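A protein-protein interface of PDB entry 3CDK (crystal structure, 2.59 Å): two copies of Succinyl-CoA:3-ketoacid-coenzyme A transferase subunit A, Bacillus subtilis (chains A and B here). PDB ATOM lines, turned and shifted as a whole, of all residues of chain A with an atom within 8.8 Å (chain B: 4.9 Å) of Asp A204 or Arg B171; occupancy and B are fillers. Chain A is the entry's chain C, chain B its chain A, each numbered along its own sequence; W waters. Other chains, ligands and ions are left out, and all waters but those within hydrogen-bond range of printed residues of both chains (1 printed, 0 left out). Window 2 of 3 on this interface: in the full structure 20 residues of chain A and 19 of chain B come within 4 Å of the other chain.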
ATOM      1  N   LEU A 168       6.740 -12.539  10.755  1.00  0.00           N
ATOM      2  CA  LEU A 168       5.869 -11.508  10.165  1.00  0.00           C
ATOM      3  C   LEU A 168       5.822 -10.166  10.878  1.00  0.00           C
ATOM      4  O   LEU A 168       5.792 -10.082  12.108  1.00  0.00           O
ATOM      5  CB  LEU A 168       4.433 -12.014   9.983  1.00  0.00           C
ATOM      6  CG  LEU A 168       4.299 -13.467   9.580  1.00  0.00           C
ATOM      7  CD1 LEU A 168       2.839 -13.859   9.603  1.00  0.00           C
ATOM      8  CD2 LEU A 168       4.896 -13.640   8.207  1.00  0.00           C
ATOM      9  N   ILE A 169       5.824  -9.115  10.064  1.00  0.00           N
ATOM     10  CA  ILE A 169       5.551  -7.751  10.507  1.00  0.00           C
ATOM     11  C   ILE A 169       4.292  -7.262   9.779  1.00  0.00           C
ATOM     12  O   ILE A 169       4.129  -7.498   8.581  1.00  0.00           O
ATOM     13  CB  ILE A 169       6.736  -6.817  10.214  1.00  0.00           C
ATOM     14  CG1 ILE A 169       7.929  -7.209  11.072  1.00  0.00           C
ATOM     15  CG2 ILE A 169       6.353  -5.368  10.474  1.00  0.00           C
ATOM     16  CD1 ILE A 169       9.212  -6.361  10.858  1.00  0.00           C
ATOM     17  N   ARG A 175      -3.068  -5.215  10.761  1.00  0.00           N
ATOM     18  CA  ARG A 175      -2.719  -6.326  11.663  1.00  0.00           C
ATOM     19  C   ARG A 175      -3.971  -7.032  12.131  1.00  0.00           C
ATOM     20  O   ARG A 175      -4.129  -8.220  11.877  1.00  0.00           O
ATOM     21  CB  ARG A 175      -2.013  -5.707  12.860  1.00  0.00           C
ATOM     22  CG  ARG A 175      -1.249  -6.539  13.908  1.00  0.00           C
ATOM     23  CD  ARG A 175      -0.493  -5.391  14.530  1.00  0.00           C
ATOM     24  NE  ARG A 175       0.278  -5.634  15.733  1.00  0.00           N
ATOM     25  CZ  ARG A 175       1.326  -4.906  16.092  1.00  0.00           C
ATOM     26  NH1 ARG A 175       1.731  -3.895  15.342  1.00  0.00           N
ATOM     27  NH2 ARG A 175       1.961  -5.202  17.208  1.00  0.00           N
ATOM     28  N   LEU A 201      14.786  -9.102   9.289  1.00  0.00           N
ATOM     29  CA  LEU A 201      13.838  -8.477  10.202  1.00  0.00           C
ATOM     30  C   LEU A 201      14.323  -8.456  11.654  1.00  0.00           C
ATOM     31  O   LEU A 201      14.674  -9.507  12.215  1.00  0.00           O
ATOM     32  CB  LEU A 201      12.486  -9.162  10.106  1.00  0.00           C
ATOM     33  CG  LEU A 201      11.887  -9.333   8.716  1.00  0.00           C
ATOM     34  CD1 LEU A 201      10.702 -10.273   8.822  1.00  0.00           C
ATOM     35  CD2 LEU A 201      11.494  -7.999   8.067  1.00  0.00           C
ATOM     36  N   ASP A 202      14.314  -7.259  12.250  1.00  0.00           N
ATOM     37  CA  ASP A 202      14.666  -7.081  13.659  1.00  0.00           C
ATOM     38  C   ASP A 202      13.800  -7.931  14.593  1.00  0.00           C
ATOM     39  O   ASP A 202      12.571  -7.795  14.621  1.00  0.00           O
ATOM     40  CB  ASP A 202      14.617  -5.610  14.090  1.00  0.00           C
ATOM     41  CG  ASP A 202      15.303  -5.376  15.443  1.00  0.00           C
ATOM     42  OD1 ASP A 202      16.554  -5.503  15.533  1.00  0.00           O
ATOM     43  OD2 ASP A 202      14.591  -5.079  16.427  1.00  0.00           O
ATOM     44  N   PRO A 203      14.451  -8.801  15.373  1.00  0.00           N
ATOM     45  CA  PRO A 203      13.772  -9.732  16.273  1.00  0.00           C
ATOM     46  C   PRO A 203      12.793  -9.036  17.228  1.00  0.00           C
ATOM     47  O   PRO A 203      11.769  -9.622  17.589  1.00  0.00           O
ATOM     48  CB  PRO A 203      14.930 -10.369  17.042  1.00  0.00           C
ATOM     49  CG  PRO A 203      16.084 -10.257  16.144  1.00  0.00           C
ATOM     50  CD  PRO A 203      15.917  -8.939  15.445  1.00  0.00           C
ATOM     51  N   ASP A 204      13.100  -7.800  17.630  1.00  0.00           N
ATOM     52  CA  ASP A 204      12.201  -7.041  18.503  1.00  0.00           C
ATOM     53  C   ASP A 204      11.112  -6.270  17.754  1.00  0.00           C
ATOM     54  O   ASP A 204      10.323  -5.577  18.389  1.00  0.00           O
ATOM     55  CB  ASP A 204      12.970  -6.099  19.422  1.00  0.00           C
ATOM     56  CG  ASP A 204      13.384  -6.761  20.753  1.00  0.00           C
ATOM     57  OD1 ASP A 204      12.590  -7.471  21.409  1.00  0.00           O
ATOM     58  OD2 ASP A 204      14.528  -6.551  21.168  1.00  0.00           O
ATOM     59  N   HIS A 205      11.063  -6.391  16.425  1.00  0.00           N
ATOM     60  CA  HIS A 205      10.029  -5.757  15.612  1.00  0.00           C
ATOM     61  C   HIS A 205       9.020  -6.793  15.142  1.00  0.00           C
ATOM     62  O   HIS A 205       7.905  -6.474  14.786  1.00  0.00           O
ATOM     63  CB  HIS A 205      10.648  -5.110  14.359  1.00  0.00           C
ATOM     64  CG  HIS A 205      11.452  -3.879  14.631  1.00  0.00           C
ATOM     65  ND1 HIS A 205      12.307  -3.766  15.707  1.00  0.00           N
ATOM     66  CD2 HIS A 205      11.565  -2.721  13.939  1.00  0.00           C
ATOM     67  CE1 HIS A 205      12.894  -2.576  15.681  1.00  0.00           C
ATOM     68  NE2 HIS A 205      12.449  -1.920  14.629  1.00  0.00           N
ATOM     69  N   ILE A 206       9.451  -8.041  15.098  1.00  0.00           N
ATOM     70  CA  ILE A 206       8.624  -9.145  14.649  1.00  0.00           C
ATOM     71  C   ILE A 206       7.327  -9.230  15.416  1.00  0.00           C
ATOM     72  O   ILE A 206       7.349  -9.172  16.631  1.00  0.00           O
ATOM     73  CB  ILE A 206       9.428 -10.449  14.716  1.00  0.00           C
ATOM     74  CG1 ILE A 206      10.505 -10.356  13.605  1.00  0.00           C
ATOM     75  CG2 ILE A 206       8.497 -11.674  14.584  1.00  0.00           C
ATOM     76  CD1 ILE A 206      11.688 -11.255  13.749  1.00  0.00           C
ATOM     77  N   HIS A 207       6.193  -9.332  14.714  1.00  0.00           N
ATOM     78  CA  HIS A 207       4.895  -9.398  15.381  1.00  0.00           C
ATOM     79  C   HIS A 207       4.398 -10.825  15.559  1.00  0.00           C
ATOM     80  O   HIS A 207       3.886 -11.187  16.638  1.00  0.00           O
ATOM     81  CB  HIS A 207       3.859  -8.545  14.653  1.00  0.00           C
ATOM     82  CG  HIS A 207       4.166  -7.075  14.673  1.00  0.00           C
ATOM     83  ND1 HIS A 207       4.127  -6.288  13.540  1.00  0.00           N
ATOM     84  CD2 HIS A 207       4.535  -6.253  15.682  1.00  0.00           C
ATOM     85  CE1 HIS A 207       4.424  -5.037  13.855  1.00  0.00           C
ATOM     86  NE2 HIS A 207       4.673  -4.992  15.152  1.00  0.00           N
ATOM     87  N   TRP B 160      12.773  -0.705  28.164  1.00  0.00           N
ATOM     88  CA  TRP B 160      13.893  -0.077  27.452  1.00  0.00           C
ATOM     89  C   TRP B 160      13.607   1.416  27.229  1.00  0.00           C
ATOM     90  O   TRP B 160      14.402   2.286  27.610  1.00  0.00           O
ATOM     91  CB  TRP B 160      14.177  -0.796  26.129  1.00  0.00           C
ATOM     92  CG  TRP B 160      15.375  -0.255  25.472  1.00  0.00           C
ATOM     93  CD1 TRP B 160      16.519   0.168  26.090  1.00  0.00           C
ATOM     94  CD2 TRP B 160      15.581  -0.063  24.067  1.00  0.00           C
ATOM     95  NE1 TRP B 160      17.415   0.627  25.155  1.00  0.00           N
ATOM     96  CE2 TRP B 160      16.869   0.490  23.906  1.00  0.00           C
ATOM     97  CE3 TRP B 160      14.806  -0.304  22.929  1.00  0.00           C
ATOM     98  CZ2 TRP B 160      17.400   0.804  22.650  1.00  0.00           C
ATOM     99  CZ3 TRP B 160      15.324   0.012  21.683  1.00  0.00           C
ATOM    100  CH2 TRP B 160      16.616   0.561  21.552  1.00  0.00           C
ATOM    101  N   ILE B 169       8.501   0.281  24.969  1.00  0.00           N
ATOM    102  CA  ILE B 169       9.158  -0.739  24.150  1.00  0.00           C
ATOM    103  C   ILE B 169      10.156  -1.478  25.034  1.00  0.00           C
ATOM    104  O   ILE B 169      10.775  -0.881  25.919  1.00  0.00           O
ATOM    105  CB  ILE B 169       9.844  -0.166  22.904  1.00  0.00           C
ATOM    106  CG1 ILE B 169      10.630  -1.252  22.164  1.00  0.00           C
ATOM    107  CG2 ILE B 169      10.846   0.927  23.292  1.00  0.00           C
ATOM    108  CD1 ILE B 169      11.478  -0.698  20.924  1.00  0.00           C
ATOM    109  N   PHE B 170      10.294  -2.781  24.799  1.00  0.00           N
ATOM    110  CA  PHE B 170      11.219  -3.618  25.553  1.00  0.00           C
ATOM    111  C   PHE B 170      12.349  -4.126  24.685  1.00  0.00           C
ATOM    112  O   PHE B 170      12.387  -3.870  23.480  1.00  0.00           O
ATOM    113  CB  PHE B 170      10.476  -4.797  26.195  1.00  0.00           C
ATOM    114  CG  PHE B 170       9.314  -4.379  27.035  1.00  0.00           C
ATOM    115  CD1 PHE B 170       8.048  -4.273  26.479  1.00  0.00           C
ATOM    116  CD2 PHE B 170       9.490  -4.054  28.368  1.00  0.00           C
ATOM    117  CE1 PHE B 170       6.969  -3.871  27.243  1.00  0.00           C
ATOM    118  CE2 PHE B 170       8.418  -3.656  29.142  1.00  0.00           C
ATOM    119  CZ  PHE B 170       7.146  -3.568  28.579  1.00  0.00           C
ATOM    120  N   ARG B 171      13.272  -4.856  25.301  1.00  0.00           N
ATOM    121  CA  ARG B 171      14.539  -5.154  24.671  1.00  0.00           C
ATOM    122  C   ARG B 171      14.919  -6.602  24.938  1.00  0.00           C
ATOM    123  O   ARG B 171      15.042  -7.012  26.088  1.00  0.00           O
ATOM    124  CB  ARG B 171      15.619  -4.207  25.204  1.00  0.00           C
ATOM    125  CG  ARG B 171      16.655  -3.827  24.183  1.00  0.00           C
ATOM    126  CD  ARG B 171      17.823  -3.057  24.786  1.00  0.00           C
ATOM    127  NE  ARG B 171      19.005  -3.904  24.885  1.00  0.00           N
ATOM    128  CZ  ARG B 171      19.762  -4.229  23.846  1.00  0.00           C
ATOM    129  NH1 ARG B 171      19.457  -3.765  22.645  1.00  0.00           N
ATOM    130  NH2 ARG B 171      20.817  -5.011  24.002  1.00  0.00           N
ATOM    131  N   LYS B 172      15.098  -7.372  23.870  1.00  0.00           N
ATOM    132  CA  LYS B 172      15.476  -8.777  23.977  1.00  0.00           C
ATOM    133  C   LYS B 172      14.599  -9.512  24.974  1.00  0.00           C
ATOM    134  O   LYS B 172      13.374  -9.388  24.937  1.00  0.00           O
ATOM    135  CB  LYS B 172      16.953  -8.920  24.367  1.00  0.00           C
ATOM    136  CG  LYS B 172      17.861  -7.982  23.632  1.00  0.00           C
ATOM    137  CD  LYS B 172      19.156  -8.681  23.242  1.00  0.00           C
ATOM    138  CE  LYS B 172      19.960  -7.863  22.185  1.00  0.00           C
ATOM    139  NZ  LYS B 172      19.217  -7.816  20.847  1.00  0.00           N
ATOM    140  N   THR B 173      15.220 -10.283  25.865  1.00  0.00           N
ATOM    141  CA  THR B 173      14.454 -11.125  26.780  1.00  0.00           C
ATOM    142  C   THR B 173      14.104 -10.389  28.069  1.00  0.00           C
ATOM    143  O   THR B 173      13.456 -10.950  28.948  1.00  0.00           O
ATOM    144  CB  THR B 173      15.200 -12.423  27.113  1.00  0.00           C
ATOM    145  OG1 THR B 173      16.531 -12.106  27.515  1.00  0.00           O
ATOM    146  CG2 THR B 173      15.250 -13.315  25.907  1.00  0.00           C
ATOM    147  N   ALA B 174      14.528  -9.130  28.164  1.00  0.00           N
ATOM    148  CA  ALA B 174      14.048  -8.230  29.226  1.00  0.00           C
ATOM    149  C   ALA B 174      12.560  -7.941  29.184  1.00  0.00           C
ATOM    150  O   ALA B 174      12.036  -7.365  30.109  1.00  0.00           O
ATOM    151  CB  ALA B 174      14.830  -6.946  29.295  1.00  0.00           C
ATOM    152  N   ARG B 175      11.886  -8.396  28.142  1.00  0.00           N
ATOM    153  CA  ARG B 175      10.418  -8.235  27.956  1.00  0.00           C
ATOM    154  C   ARG B 175       9.581  -9.108  28.897  1.00  0.00           C
ATOM    155  O   ARG B 175       8.825  -8.580  29.717  1.00  0.00           O
ATOM    156  CB  ARG B 175      10.103  -8.587  26.543  1.00  0.00           C
ATOM    157  CG  ARG B 175       8.695  -8.454  26.096  1.00  0.00           C
ATOM    158  CD  ARG B 175       8.928  -7.956  24.713  1.00  0.00           C
ATOM    159  NE  ARG B 175       7.990  -8.380  23.734  1.00  0.00           N
ATOM    160  CZ  ARG B 175       8.191  -8.255  22.431  1.00  0.00           C
ATOM    161  NH1 ARG B 175       9.330  -7.761  21.952  1.00  0.00           N
ATOM    162  NH2 ARG B 175       7.254  -8.662  21.603  1.00  0.00           N
ATOM    163  N   HIS B 207       5.431  -1.892  22.247  1.00  0.00           N
ATOM    164  CA  HIS B 207       4.998  -3.189  22.755  1.00  0.00           C
ATOM    165  C   HIS B 207       3.853  -3.157  23.745  1.00  0.00           C
ATOM    166  O   HIS B 207       3.025  -4.076  23.763  1.00  0.00           O
ATOM    167  CB  HIS B 207       6.158  -3.944  23.384  1.00  0.00           C
ATOM    168  CG  HIS B 207       7.196  -4.353  22.397  1.00  0.00           C
ATOM    169  ND1 HIS B 207       8.536  -4.078  22.574  1.00  0.00           N
ATOM    170  CD2 HIS B 207       7.085  -4.998  21.215  1.00  0.00           C
ATOM    171  CE1 HIS B 207       9.212  -4.552  21.543  1.00  0.00           C
ATOM    172  NE2 HIS B 207       8.356  -5.122  20.708  1.00  0.00           N
HETATM  173  O   HOH W   1      11.695  -7.511  24.088  1.00  0.00           O
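N of Lys B172 is in hydrogen-bond range of OD2 of Asp A204 (2.9 Å).
NH1 of Arg B175 lies within salt-bridge range of OD1 of Asp A204.
The backbone carbonyl oxygen of Asp A204 lies within hydrogen-bond range of a ring nitrogen (NE2) of His B207 (3.1 Å).
A ring nitrogen (ND1) of His B207 lies within hydrogen-bond range of the backbone NH (N) of Phe B170, at 3.1 Å.
The guanidinium group of Arg B175 sits at hydrogen-bond distance from a ring nitrogen (NE2) of His B207 (3.1 Å).
The backbone NH (N) of Asp A204 sits close to the side-chain carboxylate (OD2) of Asp A202 (3.3 Å).
Among the printed residues, pairs that only touch across the chains: Asp A204 with Arg B171 (3.8 Å).
Arg B171 touches just one residue of chain A: Asp A204 (3.8 Å).
Of chain A, only Asp A204 comes within 4 Å of Lys B172.
Of the printed residues of chain A, His B207 touches Asp A204 (3.1 Å).
Of the printed residues of chain A, Arg B175 touches Asp A204.
Leu A168 touches none of the printed residues of chain B.
The nearest printed residue of chain A that does not touch His B207 is His A205 (5.2 Å).
Of the 9 printed residues of chain B, 4 touch a printed residue of chain A.
Printed residues of chain B that touch a printed residue of chain A: Arg B171, Lys B172, Arg B175 and His B207.
Hydrophobic or aromatic side chains of chain B that line the printed part of chain A: His B207.
Among the printed residues, 4 pairs touch across the chains.
Positions printed for both chains: 169, 175 and 207.
Water W1 lies within hydrogen-bond range of the backbone carbonyl oxygen (O) of Lys B172 (2.7 Å), the side-chain carboxylate (OD1) of Asp A204 (2.8 Å), the guanidinium group (NH1) of Arg B175 (3.2 Å) and the backbone NH (N) of Arg B171 (3.3 Å).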
